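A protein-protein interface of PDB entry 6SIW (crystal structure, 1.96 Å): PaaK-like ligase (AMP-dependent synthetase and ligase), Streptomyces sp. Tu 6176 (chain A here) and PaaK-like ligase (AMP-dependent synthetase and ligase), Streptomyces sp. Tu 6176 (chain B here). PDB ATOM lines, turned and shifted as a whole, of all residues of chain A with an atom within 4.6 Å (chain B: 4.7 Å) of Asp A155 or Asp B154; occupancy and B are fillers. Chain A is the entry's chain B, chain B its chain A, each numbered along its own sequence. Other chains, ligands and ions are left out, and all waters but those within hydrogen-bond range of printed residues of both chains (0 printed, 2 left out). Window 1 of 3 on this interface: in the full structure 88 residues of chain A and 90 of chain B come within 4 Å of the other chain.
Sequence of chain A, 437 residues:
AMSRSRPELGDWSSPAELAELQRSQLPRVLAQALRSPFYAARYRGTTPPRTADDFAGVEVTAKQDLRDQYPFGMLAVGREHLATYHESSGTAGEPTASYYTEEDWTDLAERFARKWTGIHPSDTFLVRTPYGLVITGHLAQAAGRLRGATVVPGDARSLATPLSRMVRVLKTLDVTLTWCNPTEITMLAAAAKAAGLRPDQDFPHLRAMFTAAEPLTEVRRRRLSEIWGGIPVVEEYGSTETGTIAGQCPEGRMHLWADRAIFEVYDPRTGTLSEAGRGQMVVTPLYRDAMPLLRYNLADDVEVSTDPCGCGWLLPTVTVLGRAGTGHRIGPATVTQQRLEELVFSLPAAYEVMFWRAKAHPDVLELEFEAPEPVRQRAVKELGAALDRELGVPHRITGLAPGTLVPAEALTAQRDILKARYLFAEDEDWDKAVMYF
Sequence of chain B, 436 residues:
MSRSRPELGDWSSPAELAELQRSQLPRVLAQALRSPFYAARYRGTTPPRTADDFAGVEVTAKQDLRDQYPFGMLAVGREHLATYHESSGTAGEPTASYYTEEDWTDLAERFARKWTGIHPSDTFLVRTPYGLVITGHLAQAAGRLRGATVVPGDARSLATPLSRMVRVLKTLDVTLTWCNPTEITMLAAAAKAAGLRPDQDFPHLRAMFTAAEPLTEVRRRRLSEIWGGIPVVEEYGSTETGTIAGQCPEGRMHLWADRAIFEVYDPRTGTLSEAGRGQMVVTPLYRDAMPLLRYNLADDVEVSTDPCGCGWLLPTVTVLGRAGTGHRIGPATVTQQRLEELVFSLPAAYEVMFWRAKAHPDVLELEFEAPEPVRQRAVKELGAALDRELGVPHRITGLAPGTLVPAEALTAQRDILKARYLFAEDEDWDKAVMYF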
ATOM      1  N   VAL A 127     -31.958  28.957 -18.085  1.00  0.00           N
ATOM      2  CA  VAL A 127     -30.785  29.417 -18.884  1.00  0.00           C
ATOM      3  C   VAL A 127     -31.329  30.083 -20.152  1.00  0.00           C
ATOM      4  O   VAL A 127     -31.798  29.358 -21.057  1.00  0.00           O
ATOM      5  CB  VAL A 127     -29.848  28.238 -19.171  1.00  0.00           C
ATOM      6  CG1 VAL A 127     -28.704  28.615 -20.093  1.00  0.00           C
ATOM      7  CG2 VAL A 127     -29.312  27.675 -17.859  1.00  0.00           C
ATOM      8  N   ARG A 128     -31.265  31.422 -20.197  1.00  0.00           N
ATOM      9  CA  ARG A 128     -31.855  32.248 -21.276  1.00  0.00           C
ATOM     10  C   ARG A 128     -30.723  33.009 -21.965  1.00  0.00           C
ATOM     11  O   ARG A 128     -30.782  34.233 -22.062  1.00  0.00           O
ATOM     12  CB  ARG A 128     -32.970  33.131 -20.709  1.00  0.00           C
ATOM     13  CG  ARG A 128     -34.212  33.237 -21.597  1.00  0.00           C
ATOM     14  CD  ARG A 128     -33.894  33.729 -22.968  1.00  0.00           C
ATOM     15  NE  ARG A 128     -34.993  34.383 -23.672  1.00  0.00           N
ATOM     16  CZ  ARG A 128     -35.743  33.832 -24.618  1.00  0.00           C
ATOM     17  NH1 ARG A 128     -35.615  32.550 -24.931  1.00  0.00           N
ATOM     18  NH2 ARG A 128     -36.671  34.557 -25.217  1.00  0.00           N
ATOM     19  N   THR A 129     -29.721  32.271 -22.432  1.00  0.00           N
ATOM     20  CA  THR A 129     -28.618  32.769 -23.283  1.00  0.00           C
ATOM     21  C   THR A 129     -28.422  31.774 -24.416  1.00  0.00           C
ATOM     22  O   THR A 129     -28.961  30.678 -24.370  1.00  0.00           O
ATOM     23  CB  THR A 129     -27.318  32.988 -22.494  1.00  0.00           C
ATOM     24  OG1 THR A 129     -26.855  31.711 -22.038  1.00  0.00           O
ATOM     25  CG2 THR A 129     -27.494  33.955 -21.342  1.00  0.00           C
ATOM     26  N   PRO A 130     -27.741  32.155 -25.514  1.00  0.00           N
ATOM     27  CA  PRO A 130     -27.628  31.262 -26.667  1.00  0.00           C
ATOM     28  C   PRO A 130     -26.782  30.009 -26.399  1.00  0.00           C
ATOM     29  O   PRO A 130     -25.826  30.056 -25.618  1.00  0.00           O
ATOM     30  CB  PRO A 130     -26.986  32.140 -27.755  1.00  0.00           C
ATOM     31  CG  PRO A 130     -27.245  33.568 -27.289  1.00  0.00           C
ATOM     32  CD  PRO A 130     -27.206  33.498 -25.780  1.00  0.00           C
ATOM     33  N   TYR A 131     -27.155  28.918 -27.062  1.00  0.00           N
ATOM     34  CA  TYR A 131     -26.387  27.654 -27.116  1.00  0.00           C
ATOM     35  C   TYR A 131     -25.696  27.475 -28.473  1.00  0.00           C
ATOM     36  O   TYR A 131     -24.962  26.475 -28.653  1.00  0.00           O
ATOM     37  CB  TYR A 131     -27.337  26.488 -26.859  1.00  0.00           C
ATOM     38  CG  TYR A 131     -27.763  26.304 -25.425  1.00  0.00           C
ATOM     39  CD1 TYR A 131     -28.746  27.111 -24.877  1.00  0.00           C
ATOM     40  CD2 TYR A 131     -27.221  25.298 -24.624  1.00  0.00           C
ATOM     41  CE1 TYR A 131     -29.206  26.917 -23.583  1.00  0.00           C
ATOM     42  CE2 TYR A 131     -27.666  25.099 -23.322  1.00  0.00           C
ATOM     43  CZ  TYR A 131     -28.670  25.905 -22.809  1.00  0.00           C
ATOM     44  OH  TYR A 131     -29.151  25.723 -21.544  1.00  0.00           O
ATOM     45  N   GLY A 132     -25.902  28.399 -29.403  1.00  0.00           N
ATOM     46  CA  GLY A 132     -25.355  28.346 -30.776  1.00  0.00           C
ATOM     47  C   GLY A 132     -23.922  28.823 -30.828  1.00  0.00           C
ATOM     48  O   GLY A 132     -23.732  30.059 -30.816  1.00  0.00           O
ATOM     49  N   PRO A 153     -33.494  24.683 -20.258  1.00  0.00           N
ATOM     50  CA  PRO A 153     -32.741  25.310 -21.333  1.00  0.00           C
ATOM     51  C   PRO A 153     -33.674  26.213 -22.162  1.00  0.00           C
ATOM     52  O   PRO A 153     -34.365  25.740 -23.035  1.00  0.00           O
ATOM     53  CB  PRO A 153     -32.151  24.102 -22.060  1.00  0.00           C
ATOM     54  CG  PRO A 153     -33.229  23.052 -21.915  1.00  0.00           C
ATOM     55  CD  PRO A 153     -33.769  23.255 -20.508  1.00  0.00           C
ATOM     56  N   GLY A 154     -33.715  27.492 -21.806  1.00  0.00           N
ATOM     57  CA  GLY A 154     -34.496  28.512 -22.527  1.00  0.00           C
ATOM     58  C   GLY A 154     -33.863  28.833 -23.870  1.00  0.00           C
ATOM     59  O   GLY A 154     -34.612  29.088 -24.818  1.00  0.00           O
ATOM     60  N   ASP A 155     -32.536  28.764 -23.976  1.00  0.00           N
ATOM     61  CA  ASP A 155     -31.774  29.240 -25.165  1.00  0.00           C
ATOM     62  C   ASP A 155     -32.191  30.710 -25.320  1.00  0.00           C
ATOM     63  O   ASP A 155     -32.964  31.196 -24.480  1.00  0.00           O
ATOM     64  CB  ASP A 155     -32.043  28.315 -26.358  1.00  0.00           C
ATOM     65  CG  ASP A 155     -31.041  28.311 -27.502  1.00  0.00           C
ATOM     66  OD1 ASP A 155     -30.113  29.126 -27.497  1.00  0.00           O
ATOM     67  OD2 ASP A 155     -31.214  27.466 -28.407  1.00  0.00           O
ATOM     68  N   ALA A 156     -31.629  31.427 -26.274  1.00  0.00           N
ATOM     69  CA  ALA A 156     -31.969  32.834 -26.583  1.00  0.00           C
ATOM     70  C   ALA A 156     -31.752  32.985 -28.084  1.00  0.00           C
ATOM     71  O   ALA A 156     -30.905  32.235 -28.603  1.00  0.00           O
ATOM     72  CB  ALA A 156     -31.132  33.788 -25.768  1.00  0.00           C
ATOM     73  N   SER A 158     -33.639  32.117 -30.432  1.00  0.00           N
ATOM     74  CA  SER A 158     -34.200  30.884 -31.033  1.00  0.00           C
ATOM     75  C   SER A 158     -35.708  31.058 -31.246  1.00  0.00           C
ATOM     76  O   SER A 158     -36.407  31.508 -30.324  1.00  0.00           O
ATOM     77  CB  SER A 158     -33.907  29.697 -30.160  1.00  0.00           C
ATOM     78  OG  SER A 158     -34.771  28.620 -30.463  1.00  0.00           O
ATOM     79  N   THR A 161     -38.266  29.452 -28.528  1.00  0.00           N
ATOM     80  CA  THR A 161     -38.466  29.971 -27.150  1.00  0.00           C
ATOM     81  C   THR A 161     -38.665  31.477 -27.172  1.00  0.00           C
ATOM     82  O   THR A 161     -37.806  32.224 -26.712  1.00  0.00           O
ATOM     83  CB  THR A 161     -37.300  29.541 -26.258  1.00  0.00           C
ATOM     84  OG1 THR A 161     -36.106  29.997 -26.877  1.00  0.00           O
ATOM     85  CG2 THR A 161     -37.226  28.039 -26.087  1.00  0.00           C
ATOM     86  N   VAL B 126     -23.788  19.223 -33.835  1.00  0.00           N
ATOM     87  CA  VAL B 126     -25.186  19.079 -33.353  1.00  0.00           C
ATOM     88  C   VAL B 126     -25.994  20.258 -33.910  1.00  0.00           C
ATOM     89  O   VAL B 126     -25.813  21.400 -33.409  1.00  0.00           O
ATOM     90  CB  VAL B 126     -25.202  18.984 -31.819  1.00  0.00           C
ATOM     91  CG1 VAL B 126     -26.606  19.020 -31.238  1.00  0.00           C
ATOM     92  CG2 VAL B 126     -24.448  17.742 -31.370  1.00  0.00           C
ATOM     93  N   ARG B 127     -26.817  20.001 -34.927  1.00  0.00           N
ATOM     94  CA  ARG B 127     -27.585  21.019 -35.672  1.00  0.00           C
ATOM     95  C   ARG B 127     -29.078  20.735 -35.477  1.00  0.00           C
ATOM     96  O   ARG B 127     -29.830  20.618 -36.470  1.00  0.00           O
ATOM     97  CB  ARG B 127     -27.131  21.026 -37.134  1.00  0.00           C
ATOM     98  CG  ARG B 127     -27.046  22.422 -37.752  1.00  0.00           C
ATOM     99  CD  ARG B 127     -28.394  23.108 -37.729  1.00  0.00           C
ATOM    100  NE  ARG B 127     -28.601  24.193 -38.660  1.00  0.00           N
ATOM    101  CZ  ARG B 127     -28.328  25.477 -38.427  1.00  0.00           C
ATOM    102  NH1 ARG B 127     -27.752  25.873 -37.300  1.00  0.00           N
ATOM    103  NH2 ARG B 127     -28.595  26.352 -39.363  1.00  0.00           N
ATOM    104  N   THR B 128     -29.497  20.667 -34.217  1.00  0.00           N
ATOM    105  CA  THR B 128     -30.922  20.591 -33.801  1.00  0.00           C
ATOM    106  C   THR B 128     -31.107  21.567 -32.645  1.00  0.00           C
ATOM    107  O   THR B 128     -30.116  22.029 -32.068  1.00  0.00           O
ATOM    108  CB  THR B 128     -31.338  19.165 -33.413  1.00  0.00           C
ATOM    109  OG1 THR B 128     -30.609  18.791 -32.237  1.00  0.00           O
ATOM    110  CG2 THR B 128     -31.120  18.164 -34.530  1.00  0.00           C
ATOM    111  N   PRO B 129     -32.356  21.947 -32.307  1.00  0.00           N
ATOM    112  CA  PRO B 129     -32.575  22.958 -31.278  1.00  0.00           C
ATOM    113  C   PRO B 129     -32.154  22.535 -29.861  1.00  0.00           C
ATOM    114  O   PRO B 129     -32.289  21.382 -29.510  1.00  0.00           O
ATOM    115  CB  PRO B 129     -34.086  23.210 -31.344  1.00  0.00           C
ATOM    116  CG  PRO B 129     -34.496  22.748 -32.714  1.00  0.00           C
ATOM    117  CD  PRO B 129     -33.599  21.574 -32.997  1.00  0.00           C
ATOM    118  N   TYR B 130     -31.687  23.516 -29.083  1.00  0.00           N
ATOM    119  CA  TYR B 130     -31.461  23.410 -27.620  1.00  0.00           C
ATOM    120  C   TYR B 130     -32.558  24.135 -26.834  1.00  0.00           C
ATOM    121  O   TYR B 130     -32.524  24.071 -25.589  1.00  0.00           O
ATOM    122  CB  TYR B 130     -30.090  23.974 -27.259  1.00  0.00           C
ATOM    123  CG  TYR B 130     -28.915  23.129 -27.679  1.00  0.00           C
ATOM    124  CD1 TYR B 130     -28.490  23.106 -29.001  1.00  0.00           C
ATOM    125  CD2 TYR B 130     -28.188  22.391 -26.757  1.00  0.00           C
ATOM    126  CE1 TYR B 130     -27.367  22.400 -29.398  1.00  0.00           C
ATOM    127  CE2 TYR B 130     -27.051  21.684 -27.138  1.00  0.00           C
ATOM    128  CZ  TYR B 130     -26.632  21.705 -28.458  1.00  0.00           C
ATOM    129  OH  TYR B 130     -25.532  21.018 -28.848  1.00  0.00           O
ATOM    130  N   GLY B 131     -33.485  24.811 -27.512  1.00  0.00           N
ATOM    131  CA  GLY B 131     -34.552  25.598 -26.857  1.00  0.00           C
ATOM    132  C   GLY B 131     -35.715  24.715 -26.417  1.00  0.00           C
ATOM    133  O   GLY B 131     -36.517  24.336 -27.285  1.00  0.00           O
ATOM    134  N   PRO B 152     -21.657  22.666 -30.893  1.00  0.00           N
ATOM    135  CA  PRO B 152     -23.081  22.926 -30.715  1.00  0.00           C
ATOM    136  C   PRO B 152     -23.578  23.947 -31.749  1.00  0.00           C
ATOM    137  O   PRO B 152     -23.503  25.129 -31.494  1.00  0.00           O
ATOM    138  CB  PRO B 152     -23.146  23.448 -29.271  1.00  0.00           C
ATOM    139  CG  PRO B 152     -21.822  24.155 -29.083  1.00  0.00           C
ATOM    140  CD  PRO B 152     -20.825  23.362 -29.901  1.00  0.00           C
ATOM    141  N   GLY B 153     -24.041  23.461 -32.892  1.00  0.00           N
ATOM    142  CA  GLY B 153     -24.657  24.261 -33.969  1.00  0.00           C
ATOM    143  C   GLY B 153     -25.971  24.906 -33.530  1.00  0.00           C
ATOM    144  O   GLY B 153     -26.210  26.074 -33.889  1.00  0.00           O
ATOM    145  N   ASP B 154     -26.768  24.214 -32.717  1.00  0.00           N
ATOM    146  CA  ASP B 154     -28.154  24.628 -32.392  1.00  0.00           C
ATOM    147  C   ASP B 154     -28.868  24.695 -33.756  1.00  0.00           C
ATOM    148  O   ASP B 154     -28.217  24.379 -34.777  1.00  0.00           O
ATOM    149  CB  ASP B 154     -28.143  25.940 -31.581  1.00  0.00           C
ATOM    150  CG  ASP B 154     -29.344  26.209 -30.694  1.00  0.00           C
ATOM    151  OD1 ASP B 154     -30.342  25.496 -30.828  1.00  0.00           O
ATOM    152  OD2 ASP B 154     -29.269  27.155 -29.874  1.00  0.00           O
ATOM    153  N   ALA B 155     -30.153  24.998 -33.775  1.00  0.00           N
ATOM    154  CA  ALA B 155     -30.992  25.150 -34.981  1.00  0.00           C
ATOM    155  C   ALA B 155     -32.119  26.104 -34.610  1.00  0.00           C
ATOM    156  O   ALA B 155     -32.415  26.202 -33.400  1.00  0.00           O
ATOM    157  CB  ALA B 155     -31.522  23.817 -35.438  1.00  0.00           C
ATOM    158  N   SER B 157     -31.955  29.217 -34.562  1.00  0.00           N
ATOM    159  CA  SER B 157     -31.236  30.245 -33.775  1.00  0.00           C
ATOM    160  C   SER B 157     -30.605  31.247 -34.748  1.00  0.00           C
ATOM    161  O   SER B 157     -29.929  30.812 -35.704  1.00  0.00           O
ATOM    162  CB  SER B 157     -30.176  29.598 -32.910  1.00  0.00           C
ATOM    163  OG  SER B 157     -29.225  30.554 -32.476  1.00  0.00           O
ATOM    164  N   THR B 160     -26.600  30.937 -35.566  1.00  0.00           N
ATOM    165  CA  THR B 160     -25.972  29.879 -36.404  1.00  0.00           C
ATOM    166  C   THR B 160     -26.766  29.660 -37.684  1.00  0.00           C
ATOM    167  O   THR B 160     -27.406  28.632 -37.858  1.00  0.00           O
ATOM    168  CB  THR B 160     -25.805  28.593 -35.593  1.00  0.00           C
ATOM    169  OG1 THR B 160     -27.098  28.281 -35.082  1.00  0.00           O
ATOM    170  CG2 THR B 160     -24.801  28.782 -34.475  1.00  0.00           C
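The side-chain carboxylate (OD2) of Asp B154 lies close to the side-chain carboxylate (OD2) of Asp A155 (2.5 Å).
The backbone carbonyl oxygen (O) of Pro B152 lies close to the backbone carbonyl oxygen (O) of Tyr A131, 3.5 Å away.
The guanidinium group (NH1) of Arg B127 is in hydrogen-bond range of the backbone carbonyl oxygen (O) of Thr B160, 2.8 Å away.
OD1 of Asp B154 lies within hydrogen-bond range of N of Tyr B130 (3.0 Å).
O of Gly B153 is in hydrogen-bond range of OG1 of Thr B160.
The backbone carbonyl oxygen (O) of Val A127 sits at hydrogen-bond distance from the backbone NH (N) of Asp A155, at 3.1 Å.
The backbone carbonyl oxygen (O) of Asp A155 sits at hydrogen-bond distance from the guanidinium group (NH1) of Arg A128, 3.0 Å away.
The backbone carbonyl oxygen (O) of Thr A161 sits at hydrogen-bond distance from the guanidinium group (NH1) of Arg A128 (2.8 Å).
Tyr A131 touches Tyr B130 (CD2 to CD2, 3.7 Å).
OD2 of Asp B154 touches CB of Tyr A131 (3.6 Å).
Gly A132 touches Pro B152.
Gly A132 touches Gly B153 (CA to O, 3.9 Å).
Gly A132 touches Thr B160 (C to CG2, 3.8 Å).
Pro A153 touches Tyr B130 (CB to O, 3.5 Å).
Pro A153 touches Gly B131.
OD2 of Asp A155 touches CB of Tyr B130, at 3.8 Å.
Gly B131 touches Asp A155.
C of Gly B131 touches CG2 of Thr A161, at 3.7 Å.
Of chain B, only Tyr B130, Gly B131 and Asp B154 come within 4 Å of Asp A155.
Asp B154 touches just these residues of chain A: Tyr A131 (3.6 Å), Gly A132 (3.6 Å) and Asp A155 (2.5 Å).
Printed residues of chain A within 4 Å of Gly B131: Pro A153, Asp A155 and Thr A161.
Of the printed residues of chain B, Thr A161 touches Gly B131.
Ser B157 touches none of the printed residues of chain A.
The nearest printed residue of chain B that does not touch Asp A155 is Ser B157 (5.1 Å).
Printed residues of chain B that touch a printed residue of chain A: Tyr B130, Gly B131, Pro B152, Gly B153, Asp B154 and Thr B160.
Hydrophobic or aromatic side chains of chain A that line the printed part of chain B: Tyr A131 and Pro A153.
Along chain A the printed residues that touch a printed residue of chain B span positions 131 to 161.
Among the printed residues, no Asp or Glu carboxylate lies within 4 Å of a Lys or Arg side-chain nitrogen of the other chain.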
